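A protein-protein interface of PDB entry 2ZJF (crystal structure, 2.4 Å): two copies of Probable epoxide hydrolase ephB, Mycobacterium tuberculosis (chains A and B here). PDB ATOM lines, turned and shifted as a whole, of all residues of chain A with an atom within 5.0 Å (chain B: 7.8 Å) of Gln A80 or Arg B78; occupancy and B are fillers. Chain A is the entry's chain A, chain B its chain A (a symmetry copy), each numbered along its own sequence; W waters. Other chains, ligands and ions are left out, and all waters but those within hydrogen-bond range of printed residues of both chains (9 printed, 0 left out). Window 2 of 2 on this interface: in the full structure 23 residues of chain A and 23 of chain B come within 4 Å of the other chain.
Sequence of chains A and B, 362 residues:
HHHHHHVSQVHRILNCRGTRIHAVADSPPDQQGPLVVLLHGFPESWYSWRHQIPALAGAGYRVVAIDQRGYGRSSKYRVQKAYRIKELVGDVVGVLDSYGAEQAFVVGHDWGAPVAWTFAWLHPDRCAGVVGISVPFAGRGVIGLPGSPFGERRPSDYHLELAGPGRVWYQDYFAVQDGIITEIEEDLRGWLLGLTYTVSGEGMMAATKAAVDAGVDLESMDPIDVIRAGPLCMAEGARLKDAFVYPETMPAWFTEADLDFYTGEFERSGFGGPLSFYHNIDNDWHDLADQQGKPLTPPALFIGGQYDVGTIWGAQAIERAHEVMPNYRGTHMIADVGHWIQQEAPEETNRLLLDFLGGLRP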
ATOM      1  N   ARG A  78      -5.603  12.621  26.467  1.00  0.00           N
ATOM      2  CA  ARG A  78      -6.786  11.806  26.714  1.00  0.00           C
ATOM      3  C   ARG A  78      -8.034  12.364  26.029  1.00  0.00           C
ATOM      4  O   ARG A  78      -8.782  11.606  25.422  1.00  0.00           O
ATOM      5  CB  ARG A  78      -7.077  11.649  28.211  1.00  0.00           C
ATOM      6  CG  ARG A  78      -8.249  10.698  28.446  1.00  0.00           C
ATOM      7  CD  ARG A  78      -8.500  10.379  29.913  1.00  0.00           C
ATOM      8  NE  ARG A  78      -9.448   9.269  30.042  1.00  0.00           N
ATOM      9  CZ  ARG A  78     -10.756   9.361  29.807  1.00  0.00           C
ATOM     10  NH1 ARG A  78     -11.286  10.520  29.440  1.00  0.00           N
ATOM     11  NH2 ARG A  78     -11.533   8.286  29.913  1.00  0.00           N
ATOM     12  N   VAL A  79      -8.259  13.678  26.129  1.00  0.00           N
ATOM     13  CA  VAL A  79      -9.441  14.309  25.531  1.00  0.00           C
ATOM     14  C   VAL A  79      -9.552  14.044  24.034  1.00  0.00           C
ATOM     15  O   VAL A  79      -8.550  14.083  23.310  1.00  0.00           O
ATOM     16  CB  VAL A  79      -9.462  15.847  25.758  1.00  0.00           C
ATOM     17  CG1 VAL A  79      -9.465  16.157  27.247  1.00  0.00           C
ATOM     18  CG2 VAL A  79      -8.266  16.499  25.073  1.00  0.00           C
ATOM     19  N   GLN A  80     -10.782  13.793  23.582  1.00  0.00           N
ATOM     20  CA  GLN A  80     -11.073  13.497  22.182  1.00  0.00           C
ATOM     21  C   GLN A  80     -10.681  14.579  21.181  1.00  0.00           C
ATOM     22  O   GLN A  80     -10.271  14.267  20.064  1.00  0.00           O
ATOM     23  CB  GLN A  80     -12.565  13.188  22.008  1.00  0.00           C
ATOM     24  CG  GLN A  80     -13.066  11.999  22.820  1.00  0.00           C
ATOM     25  CD  GLN A  80     -12.493  10.670  22.353  1.00  0.00           C
ATOM     26  OE1 GLN A  80     -11.540  10.625  21.568  1.00  0.00           O
ATOM     27  NE2 GLN A  80     -13.067   9.578  22.843  1.00  0.00           N
ATOM     28  N   LYS A  81     -10.808  15.843  21.571  1.00  0.00           N
ATOM     29  CA  LYS A  81     -10.497  16.940  20.661  1.00  0.00           C
ATOM     30  C   LYS A  81      -9.033  17.025  20.228  1.00  0.00           C
ATOM     31  O   LYS A  81      -8.714  17.670  19.225  1.00  0.00           O
ATOM     32  CB  LYS A  81     -10.941  18.282  21.263  1.00  0.00           C
ATOM     33  CG  LYS A  81     -10.313  18.634  22.602  1.00  0.00           C
ATOM     34  CD  LYS A  81     -10.507  20.122  22.907  1.00  0.00           C
ATOM     35  CE  LYS A  81      -9.877  20.538  24.232  1.00  0.00           C
ATOM     36  NZ  LYS A  81     -10.655  20.035  25.409  1.00  0.00           N
ATOM     37  N   ALA A  82      -8.145  16.368  20.968  1.00  0.00           N
ATOM     38  CA  ALA A  82      -6.730  16.393  20.626  1.00  0.00           C
ATOM     39  C   ALA A  82      -6.413  15.519  19.417  1.00  0.00           C
ATOM     40  O   ALA A  82      -5.341  15.641  18.826  1.00  0.00           O
ATOM     41  CB  ALA A  82      -5.902  15.948  21.813  1.00  0.00           C
ATOM     42  N   TYR A  83      -7.352  14.656  19.037  1.00  0.00           N
ATOM     43  CA  TYR A  83      -7.143  13.747  17.910  1.00  0.00           C
ATOM     44  C   TYR A  83      -7.951  14.055  16.651  1.00  0.00           C
ATOM     45  O   TYR A  83      -8.219  13.169  15.838  1.00  0.00           O
ATOM     46  CB  TYR A  83      -7.393  12.304  18.373  1.00  0.00           C
ATOM     47  CG  TYR A  83      -6.402  11.881  19.437  1.00  0.00           C
ATOM     48  CD1 TYR A  83      -5.097  11.500  19.095  1.00  0.00           C
ATOM     49  CD2 TYR A  83      -6.729  11.958  20.790  1.00  0.00           C
ATOM     50  CE1 TYR A  83      -4.151  11.210  20.074  1.00  0.00           C
ATOM     51  CE2 TYR A  83      -5.792  11.675  21.773  1.00  0.00           C
ATOM     52  CZ  TYR A  83      -4.504  11.301  21.413  1.00  0.00           C
ATOM     53  OH  TYR A  83      -3.575  11.017  22.396  1.00  0.00           O
ATOM     54  N   ARG A  84      -8.329  15.316  16.487  1.00  0.00           N
ATOM     55  CA  ARG A  84      -9.082  15.733  15.311  1.00  0.00           C
ATOM     56  C   ARG A  84      -8.077  15.980  14.185  1.00  0.00           C
ATOM     57  O   ARG A  84      -6.905  16.260  14.449  1.00  0.00           O
ATOM     58  CB  ARG A  84      -9.887  16.987  15.629  1.00  0.00           C
ATOM     59  CG  ARG A  84     -10.841  16.765  16.791  1.00  0.00           C
ATOM     60  CD  ARG A  84     -11.546  18.035  17.208  1.00  0.00           C
ATOM     61  NE  ARG A  84     -12.644  18.374  16.311  1.00  0.00           N
ATOM     62  CZ  ARG A  84     -13.886  18.591  16.723  1.00  0.00           C
ATOM     63  NH1 ARG A  84     -14.835  18.900  15.850  1.00  0.00           N
ATOM     64  NH2 ARG A  84     -14.178  18.490  18.012  1.00  0.00           N
ATOM     65  N   GLN A 177     -13.979   2.606  21.961  1.00  0.00           N
ATOM     66  CA  GLN A 177     -12.814   2.517  22.849  1.00  0.00           C
ATOM     67  C   GLN A 177     -13.067   1.814  24.184  1.00  0.00           C
ATOM     68  O   GLN A 177     -12.583   2.241  25.226  1.00  0.00           O
ATOM     69  CB  GLN A 177     -12.261   3.924  23.112  1.00  0.00           C
ATOM     70  CG  GLN A 177     -11.648   4.590  21.883  1.00  0.00           C
ATOM     71  CD  GLN A 177     -11.457   6.091  22.050  1.00  0.00           C
ATOM     72  OE1 GLN A 177     -12.426   6.855  22.062  1.00  0.00           O
ATOM     73  NE2 GLN A 177     -10.206   6.520  22.180  1.00  0.00           N
ATOM     74  N   ILE A 181     -10.448  -2.163  23.199  1.00  0.00           N
ATOM     75  CA  ILE A 181      -9.226  -2.182  23.997  1.00  0.00           C
ATOM     76  C   ILE A 181      -9.181  -3.427  24.882  1.00  0.00           C
ATOM     77  O   ILE A 181      -8.132  -4.062  25.036  1.00  0.00           O
ATOM     78  CB  ILE A 181      -9.110  -0.903  24.864  1.00  0.00           C
ATOM     79  CG1 ILE A 181      -8.832   0.299  23.956  1.00  0.00           C
ATOM     80  CG2 ILE A 181      -7.998  -1.051  25.884  1.00  0.00           C
ATOM     81  CD1 ILE A 181      -8.858   1.623  24.658  1.00  0.00           C
ATOM     82  N   GLY A 272      -5.476   3.851  23.279  1.00  0.00           N
ATOM     83  CA  GLY A 272      -6.382   4.961  23.507  1.00  0.00           C
ATOM     84  C   GLY A 272      -6.204   6.117  22.537  1.00  0.00           C
ATOM     85  O   GLY A 272      -7.169   6.588  21.940  1.00  0.00           O
ATOM     86  N   SER A 276      -8.582   7.097  19.171  1.00  0.00           N
ATOM     87  CA  SER A 276      -9.250   8.392  19.145  1.00  0.00           C
ATOM     88  C   SER A 276      -9.240   9.006  17.755  1.00  0.00           C
ATOM     89  O   SER A 276     -10.057   9.874  17.454  1.00  0.00           O
ATOM     90  CB  SER A 276      -8.604   9.351  20.132  1.00  0.00           C
ATOM     91  OG  SER A 276      -9.049   9.067  21.442  1.00  0.00           O
ATOM     92  N   HIS A 279     -12.408   7.830  16.521  1.00  0.00           N
ATOM     93  CA  HIS A 279     -13.489   8.469  17.249  1.00  0.00           C
ATOM     94  C   HIS A 279     -13.870   9.824  16.662  1.00  0.00           C
ATOM     95  O   HIS A 279     -15.019  10.246  16.762  1.00  0.00           O
ATOM     96  CB  HIS A 279     -13.096   8.613  18.724  1.00  0.00           C
ATOM     97  CG  HIS A 279     -14.215   9.067  19.611  1.00  0.00           C
ATOM     98  ND1 HIS A 279     -14.567  10.393  19.748  1.00  0.00           N
ATOM     99  CD2 HIS A 279     -15.072   8.366  20.390  1.00  0.00           C
ATOM    100  CE1 HIS A 279     -15.593  10.489  20.576  1.00  0.00           C
ATOM    101  NE2 HIS A 279     -15.918   9.274  20.978  1.00  0.00           N
ATOM    102  N   ASN A 280     -12.913  10.490  16.023  1.00  0.00           N
ATOM    103  CA  ASN A 280     -13.156  11.814  15.449  1.00  0.00           C
ATOM    104  C   ASN A 280     -13.489  11.862  13.961  1.00  0.00           C
ATOM    105  O   ASN A 280     -13.658  12.948  13.409  1.00  0.00           O
ATOM    106  CB  ASN A 280     -11.952  12.714  15.723  1.00  0.00           C
ATOM    107  CG  ASN A 280     -11.824  13.072  17.182  1.00  0.00           C
ATOM    108  OD1 ASN A 280     -12.660  13.791  17.722  1.00  0.00           O
ATOM    109  ND2 ASN A 280     -10.781  12.565  17.836  1.00  0.00           N
ATOM    110  N   SER B  75      -1.187  -3.064  30.867  1.00  0.00           N
ATOM    111  CA  SER B  75      -2.356  -2.688  30.069  1.00  0.00           C
ATOM    112  C   SER B  75      -2.840  -1.264  30.300  1.00  0.00           C
ATOM    113  O   SER B  75      -2.982  -0.816  31.445  1.00  0.00           O
ATOM    114  CB  SER B  75      -3.513  -3.650  30.337  1.00  0.00           C
ATOM    115  OG  SER B  75      -3.220  -4.939  29.841  1.00  0.00           O
ATOM    116  N   LYS B  76      -3.100  -0.570  29.196  1.00  0.00           N
ATOM    117  CA  LYS B  76      -3.567   0.809  29.228  1.00  0.00           C
ATOM    118  C   LYS B  76      -5.029   0.888  28.793  1.00  0.00           C
ATOM    119  O   LYS B  76      -5.325   0.837  27.598  1.00  0.00           O
ATOM    120  CB  LYS B  76      -2.721   1.676  28.283  1.00  0.00           C
ATOM    121  CG  LYS B  76      -1.216   1.618  28.513  1.00  0.00           C
ATOM    122  CD  LYS B  76      -0.851   2.012  29.929  1.00  0.00           C
ATOM    123  CE  LYS B  76       0.646   2.177  30.073  1.00  0.00           C
ATOM    124  NZ  LYS B  76       1.374   0.971  29.622  1.00  0.00           N
ATOM    125  N   TYR B  77      -5.940   1.007  29.757  1.00  0.00           N
ATOM    126  CA  TYR B  77      -7.376   1.108  29.457  1.00  0.00           C
ATOM    127  C   TYR B  77      -7.786   2.569  29.357  1.00  0.00           C
ATOM    128  O   TYR B  77      -7.228   3.422  30.057  1.00  0.00           O
ATOM    129  CB  TYR B  77      -8.207   0.467  30.570  1.00  0.00           C
ATOM    130  CG  TYR B  77      -8.040  -1.019  30.700  1.00  0.00           C
ATOM    131  CD1 TYR B  77      -8.634  -1.889  29.786  1.00  0.00           C
ATOM    132  CD2 TYR B  77      -7.259  -1.559  31.717  1.00  0.00           C
ATOM    133  CE1 TYR B  77      -8.451  -3.264  29.885  1.00  0.00           C
ATOM    134  CE2 TYR B  77      -7.067  -2.933  31.826  1.00  0.00           C
ATOM    135  CZ  TYR B  77      -7.666  -3.781  30.905  1.00  0.00           C
ATOM    136  OH  TYR B  77      -7.470  -5.138  31.010  1.00  0.00           O
ATOM    137  N   ARG B  78      -8.761   2.868  28.504  1.00  0.00           N
ATOM    138  CA  ARG B  78      -9.224   4.246  28.398  1.00  0.00           C
ATOM    139  C   ARG B  78     -10.433   4.526  29.293  1.00  0.00           C
ATOM    140  O   ARG B  78     -10.463   5.550  29.966  1.00  0.00           O
ATOM    141  CB  ARG B  78      -9.583   4.624  26.957  1.00  0.00           C
ATOM    142  CG  ARG B  78      -9.955   6.103  26.853  1.00  0.00           C
ATOM    143  CD  ARG B  78     -10.179   6.584  25.427  1.00  0.00           C
ATOM    144  NE  ARG B  78     -10.263   8.046  25.385  1.00  0.00           N
ATOM    145  CZ  ARG B  78     -11.303   8.756  25.821  1.00  0.00           C
ATOM    146  NH1 ARG B  78     -12.365   8.141  26.324  1.00  0.00           N
ATOM    147  NH2 ARG B  78     -11.271  10.085  25.778  1.00  0.00           N
ATOM    148  N   VAL B  79     -11.422   3.627  29.297  1.00  0.00           N
ATOM    149  CA  VAL B  79     -12.636   3.815  30.098  1.00  0.00           C
ATOM    150  C   VAL B  79     -12.334   4.014  31.580  1.00  0.00           C
ATOM    151  O   VAL B  79     -11.466   3.337  32.144  1.00  0.00           O
ATOM    152  CB  VAL B  79     -13.622   2.621  29.957  1.00  0.00           C
ATOM    153  CG1 VAL B  79     -14.039   2.454  28.505  1.00  0.00           C
ATOM    154  CG2 VAL B  79     -12.982   1.341  30.486  1.00  0.00           C
ATOM    155  N   GLN B  80     -13.072   4.937  32.198  1.00  0.00           N
ATOM    156  CA  GLN B  80     -12.906   5.276  33.611  1.00  0.00           C
ATOM    157  C   GLN B  80     -13.106   4.129  34.595  1.00  0.00           C
ATOM    158  O   GLN B  80     -12.428   4.068  35.619  1.00  0.00           O
ATOM    159  CB  GLN B  80     -13.855   6.419  33.992  1.00  0.00           C
ATOM    160  CG  GLN B  80     -13.645   7.708  33.205  1.00  0.00           C
ATOM    161  CD  GLN B  80     -12.321   8.388  33.510  1.00  0.00           C
ATOM    162  OE1 GLN B  80     -11.432   7.804  34.138  1.00  0.00           O
ATOM    163  NE2 GLN B  80     -12.179   9.628  33.057  1.00  0.00           N
ATOM    164  N   LYS B  81     -14.033   3.225  34.295  1.00  0.00           N
ATOM    165  CA  LYS B  81     -14.319   2.119  35.203  1.00  0.00           C
ATOM    166  C   LYS B  81     -13.163   1.139  35.412  1.00  0.00           C
ATOM    167  O   LYS B  81     -13.155   0.383  36.387  1.00  0.00           O
ATOM    168  CB  LYS B  81     -15.572   1.357  34.744  1.00  0.00           C
ATOM    169  CG  LYS B  81     -15.499   0.765  33.346  1.00  0.00           C
ATOM    170  CD  LYS B  81     -16.602  -0.281  33.151  1.00  0.00           C
ATOM    171  CE  LYS B  81     -16.564  -0.923  31.770  1.00  0.00           C
ATOM    172  NZ  LYS B  81     -17.044   0.008  30.701  1.00  0.00           N
ATOM    173  N   ALA B  82     -12.185   1.158  34.511  1.00  0.00           N
ATOM    174  CA  ALA B  82     -11.045   0.261  34.636  1.00  0.00           C
ATOM    175  C   ALA B  82     -10.084   0.698  35.737  1.00  0.00           C
ATOM    176  O   ALA B  82      -9.232  -0.081  36.163  1.00  0.00           O
ATOM    177  CB  ALA B  82     -10.309   0.172  33.317  1.00  0.00           C
ATOM    178  N   TYR B  83     -10.232   1.933  36.210  1.00  0.00           N
ATOM    179  CA  TYR B  83      -9.346   2.468  37.243  1.00  0.00           C
ATOM    180  C   TYR B  83      -9.972   2.649  38.624  1.00  0.00           C
ATOM    181  O   TYR B  83      -9.519   3.473  39.421  1.00  0.00           O
ATOM    182  CB  TYR B  83      -8.734   3.787  36.749  1.00  0.00           C
ATOM    183  CG  TYR B  83      -7.866   3.575  35.525  1.00  0.00           C
ATOM    184  CD1 TYR B  83      -6.566   3.067  35.646  1.00  0.00           C
ATOM    185  CD2 TYR B  83      -8.374   3.783  34.244  1.00  0.00           C
ATOM    186  CE1 TYR B  83      -5.801   2.771  34.521  1.00  0.00           C
ATOM    187  CE2 TYR B  83      -7.621   3.488  33.117  1.00  0.00           C
ATOM    188  CZ  TYR B  83      -6.334   2.984  33.258  1.00  0.00           C
ATOM    189  OH  TYR B  83      -5.587   2.695  32.132  1.00  0.00           O
ATOM    190  N   GLN B 177      -8.518  15.661  33.704  1.00  0.00           N
ATOM    191  CA  GLN B 177      -7.691  15.070  32.646  1.00  0.00           C
ATOM    192  C   GLN B 177      -7.663  15.849  31.331  1.00  0.00           C
ATOM    193  O   GLN B 177      -7.704  15.270  30.250  1.00  0.00           O
ATOM    194  CB  GLN B 177      -8.154  13.632  32.375  1.00  0.00           C
ATOM    195  CG  GLN B 177      -7.895  12.668  33.530  1.00  0.00           C
ATOM    196  CD  GLN B 177      -8.684  11.371  33.414  1.00  0.00           C
ATOM    197  OE1 GLN B 177      -9.905  11.356  33.590  1.00  0.00           O
ATOM    198  NE2 GLN B 177      -7.989  10.277  33.119  1.00  0.00           N
ATOM    199  N   GLY B 272      -2.847   9.574  31.177  1.00  0.00           N
ATOM    200  CA  GLY B 272      -4.263   9.257  31.147  1.00  0.00           C
ATOM    201  C   GLY B 272      -4.679   8.183  32.137  1.00  0.00           C
ATOM    202  O   GLY B 272      -5.627   8.365  32.898  1.00  0.00           O
ATOM    203  N   GLY B 273      -3.975   7.057  32.128  1.00  0.00           N
ATOM    204  CA  GLY B 273      -4.302   5.981  33.042  1.00  0.00           C
ATOM    205  C   GLY B 273      -4.081   6.429  34.477  1.00  0.00           C
ATOM    206  O   GLY B 273      -5.000   6.394  35.299  1.00  0.00           O
ATOM    207  N   SER B 276      -6.618   8.677  35.872  1.00  0.00           N
ATOM    208  CA  SER B 276      -7.921   8.056  36.066  1.00  0.00           C
ATOM    209  C   SER B 276      -8.076   7.491  37.468  1.00  0.00           C
ATOM    210  O   SER B 276      -9.195   7.284  37.934  1.00  0.00           O
ATOM    211  CB  SER B 276      -8.150   6.955  35.043  1.00  0.00           C
ATOM    212  OG  SER B 276      -8.524   7.518  33.804  1.00  0.00           O
HETATM  213  O   HOH W   1     -10.197  13.060  29.233  1.00  0.00           O
HETATM  214  O   HOH W   2      -7.977   9.461  23.980  1.00  0.00           O
HETATM  215  O   HOH W   3     -14.809   9.805  24.960  1.00  0.00           O
HETATM  216  O   HOH W   4     -11.048   1.050  27.724  1.00  0.00           O
HETATM  217  O   HOH W   5     -13.995  10.616  31.244  1.00  0.00           O
HETATM  218  O   HOH W   6      -4.840   3.604  25.863  1.00  0.00           O
HETATM  219  O   HOH W   7     -13.028   5.455  26.494  1.00  0.00           O
HETATM  220  O   HOH W   8      -8.313   6.686  31.156  1.00  0.00           O
HETATM  221  O   HOH W   9      -6.163  15.411  27.491  1.00  0.00           O
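The guanidinium group of Arg A78 is in hydrogen-bond range of the backbone carbonyl oxygen of Arg B78 (2.9 Å).
NH2 of Arg A78 lies close to NE2 of Gln B80 (3.5 Å).
The guanidinium group of Arg B78 sits close to the side-chain amide nitrogen of Gln A80, at 3.5 Å.
The side-chain amide oxygen of Gln A177 sits at hydrogen-bond distance from the side-chain amide nitrogen of Gln A80.
OE1 of Gln A80 lies within hydrogen-bond range of OG of Ser A276 (2.9 Å).
The side-chain amide nitrogen (NE2) of Gln A177 lies within hydrogen-bond range of the side-chain hydroxyl (OG) of Ser A276 (2.9 Å).
The side-chain amide oxygen (OE1) of Gln B177 is in hydrogen-bond range of the side-chain amide nitrogen (NE2) of Gln B80, at 2.9 Å.
O of Gly B272 lies within hydrogen-bond range of NE2 of Gln B177 (3.0 Å).
The side-chain amide nitrogen of Gln B177 is in hydrogen-bond range of the side-chain hydroxyl of Ser B276 (2.9 Å).
Among the printed residues, merely in contact across the chains: Gln A177 with Arg B78 (3.2 Å), Arg A78 with Gln B177 (3.2 Å), Val A79 with Gln B177 (3.6 Å), Gln A177 with Val B79 (3.6 Å), Ile A181 with Lys B76 (3.7 Å) and Ile A181 with Arg B78 (3.8 Å).
Gln A80 touches just one residue of chain B: Arg B78.
Arg A84 touches none of the printed residues of chain B.
Asn A280 touches none of the printed residues of chain B.
Printed residues of chain A within 4 Å of Lys B76: Ile A181 (3.7 Å).
Arg B78 touches just these residues of chain A: Arg A78, Gln A80, Gln A177 and Ile A181.
Printed residues of chain A within 4 Å of Gln B177: Arg A78 (3.2 Å) and Val A79 (3.6 Å).
Of the 13 printed residues of chain A, 5 touch a printed residue of chain B.
Of the 13 printed residues of chain B, 5 touch a printed residue of chain A.
Among the printed residues, 9 pairs touch across the chains.
Among the printed residues, no Asp or Glu carboxylate lies within 4 Å of a Lys or Arg side-chain nitrogen of the other chain.
Arg A78 touches its own counterpart, Arg B78.
Arg A78 touches Gln B80, and with the chains exchanged Gln A80 touches Arg B78.
Arg A78 touches Gln B177, and with the chains exchanged Gln A177 touches Arg B78.
Val A79 touches Gln B177, and with the chains exchanged Gln A177 touches Val B79.
Positions printed for both chains: 78, 79, 80, 81, 82, 83, 177, 272 and 276.
Of the 9 pairs that touch across the chains among the printed residues, 7 have their exchanged pair printed and touching as well.
Water W2 lies within hydrogen-bond range of the backbone carbonyl oxygen (O) of Arg A78 (2.7 Å), the side-chain hydroxyl (OG) of Ser A276 (2.8 Å) and the guanidinium group (NE) of Arg B78 (3.0 Å).
Water W8 lies within hydrogen-bond range of the backbone carbonyl oxygen (O) of Arg B78 (2.7 Å), the side-chain hydroxyl (OG) of Ser B276 (2.8 Å) and the guanidinium group (NE) of Arg A78 (3.0 Å).
Water W3 bridges NE2 of Gln A80 (2.8 Å) and NH1 of Arg B78 (3.3 Å).
Water W5 bridges NE2 of Gln B80 and NH1 of Arg A78.
Water W1 bridges NH1 of Arg A78 (2.8 Å) and O of Gln B177 (3.5 Å).
Water W9 lies within hydrogen-bond range of N of Arg A78 (3.0 Å), N of Val A79 (3.0 Å) and O of Gln B177 (3.2 Å).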
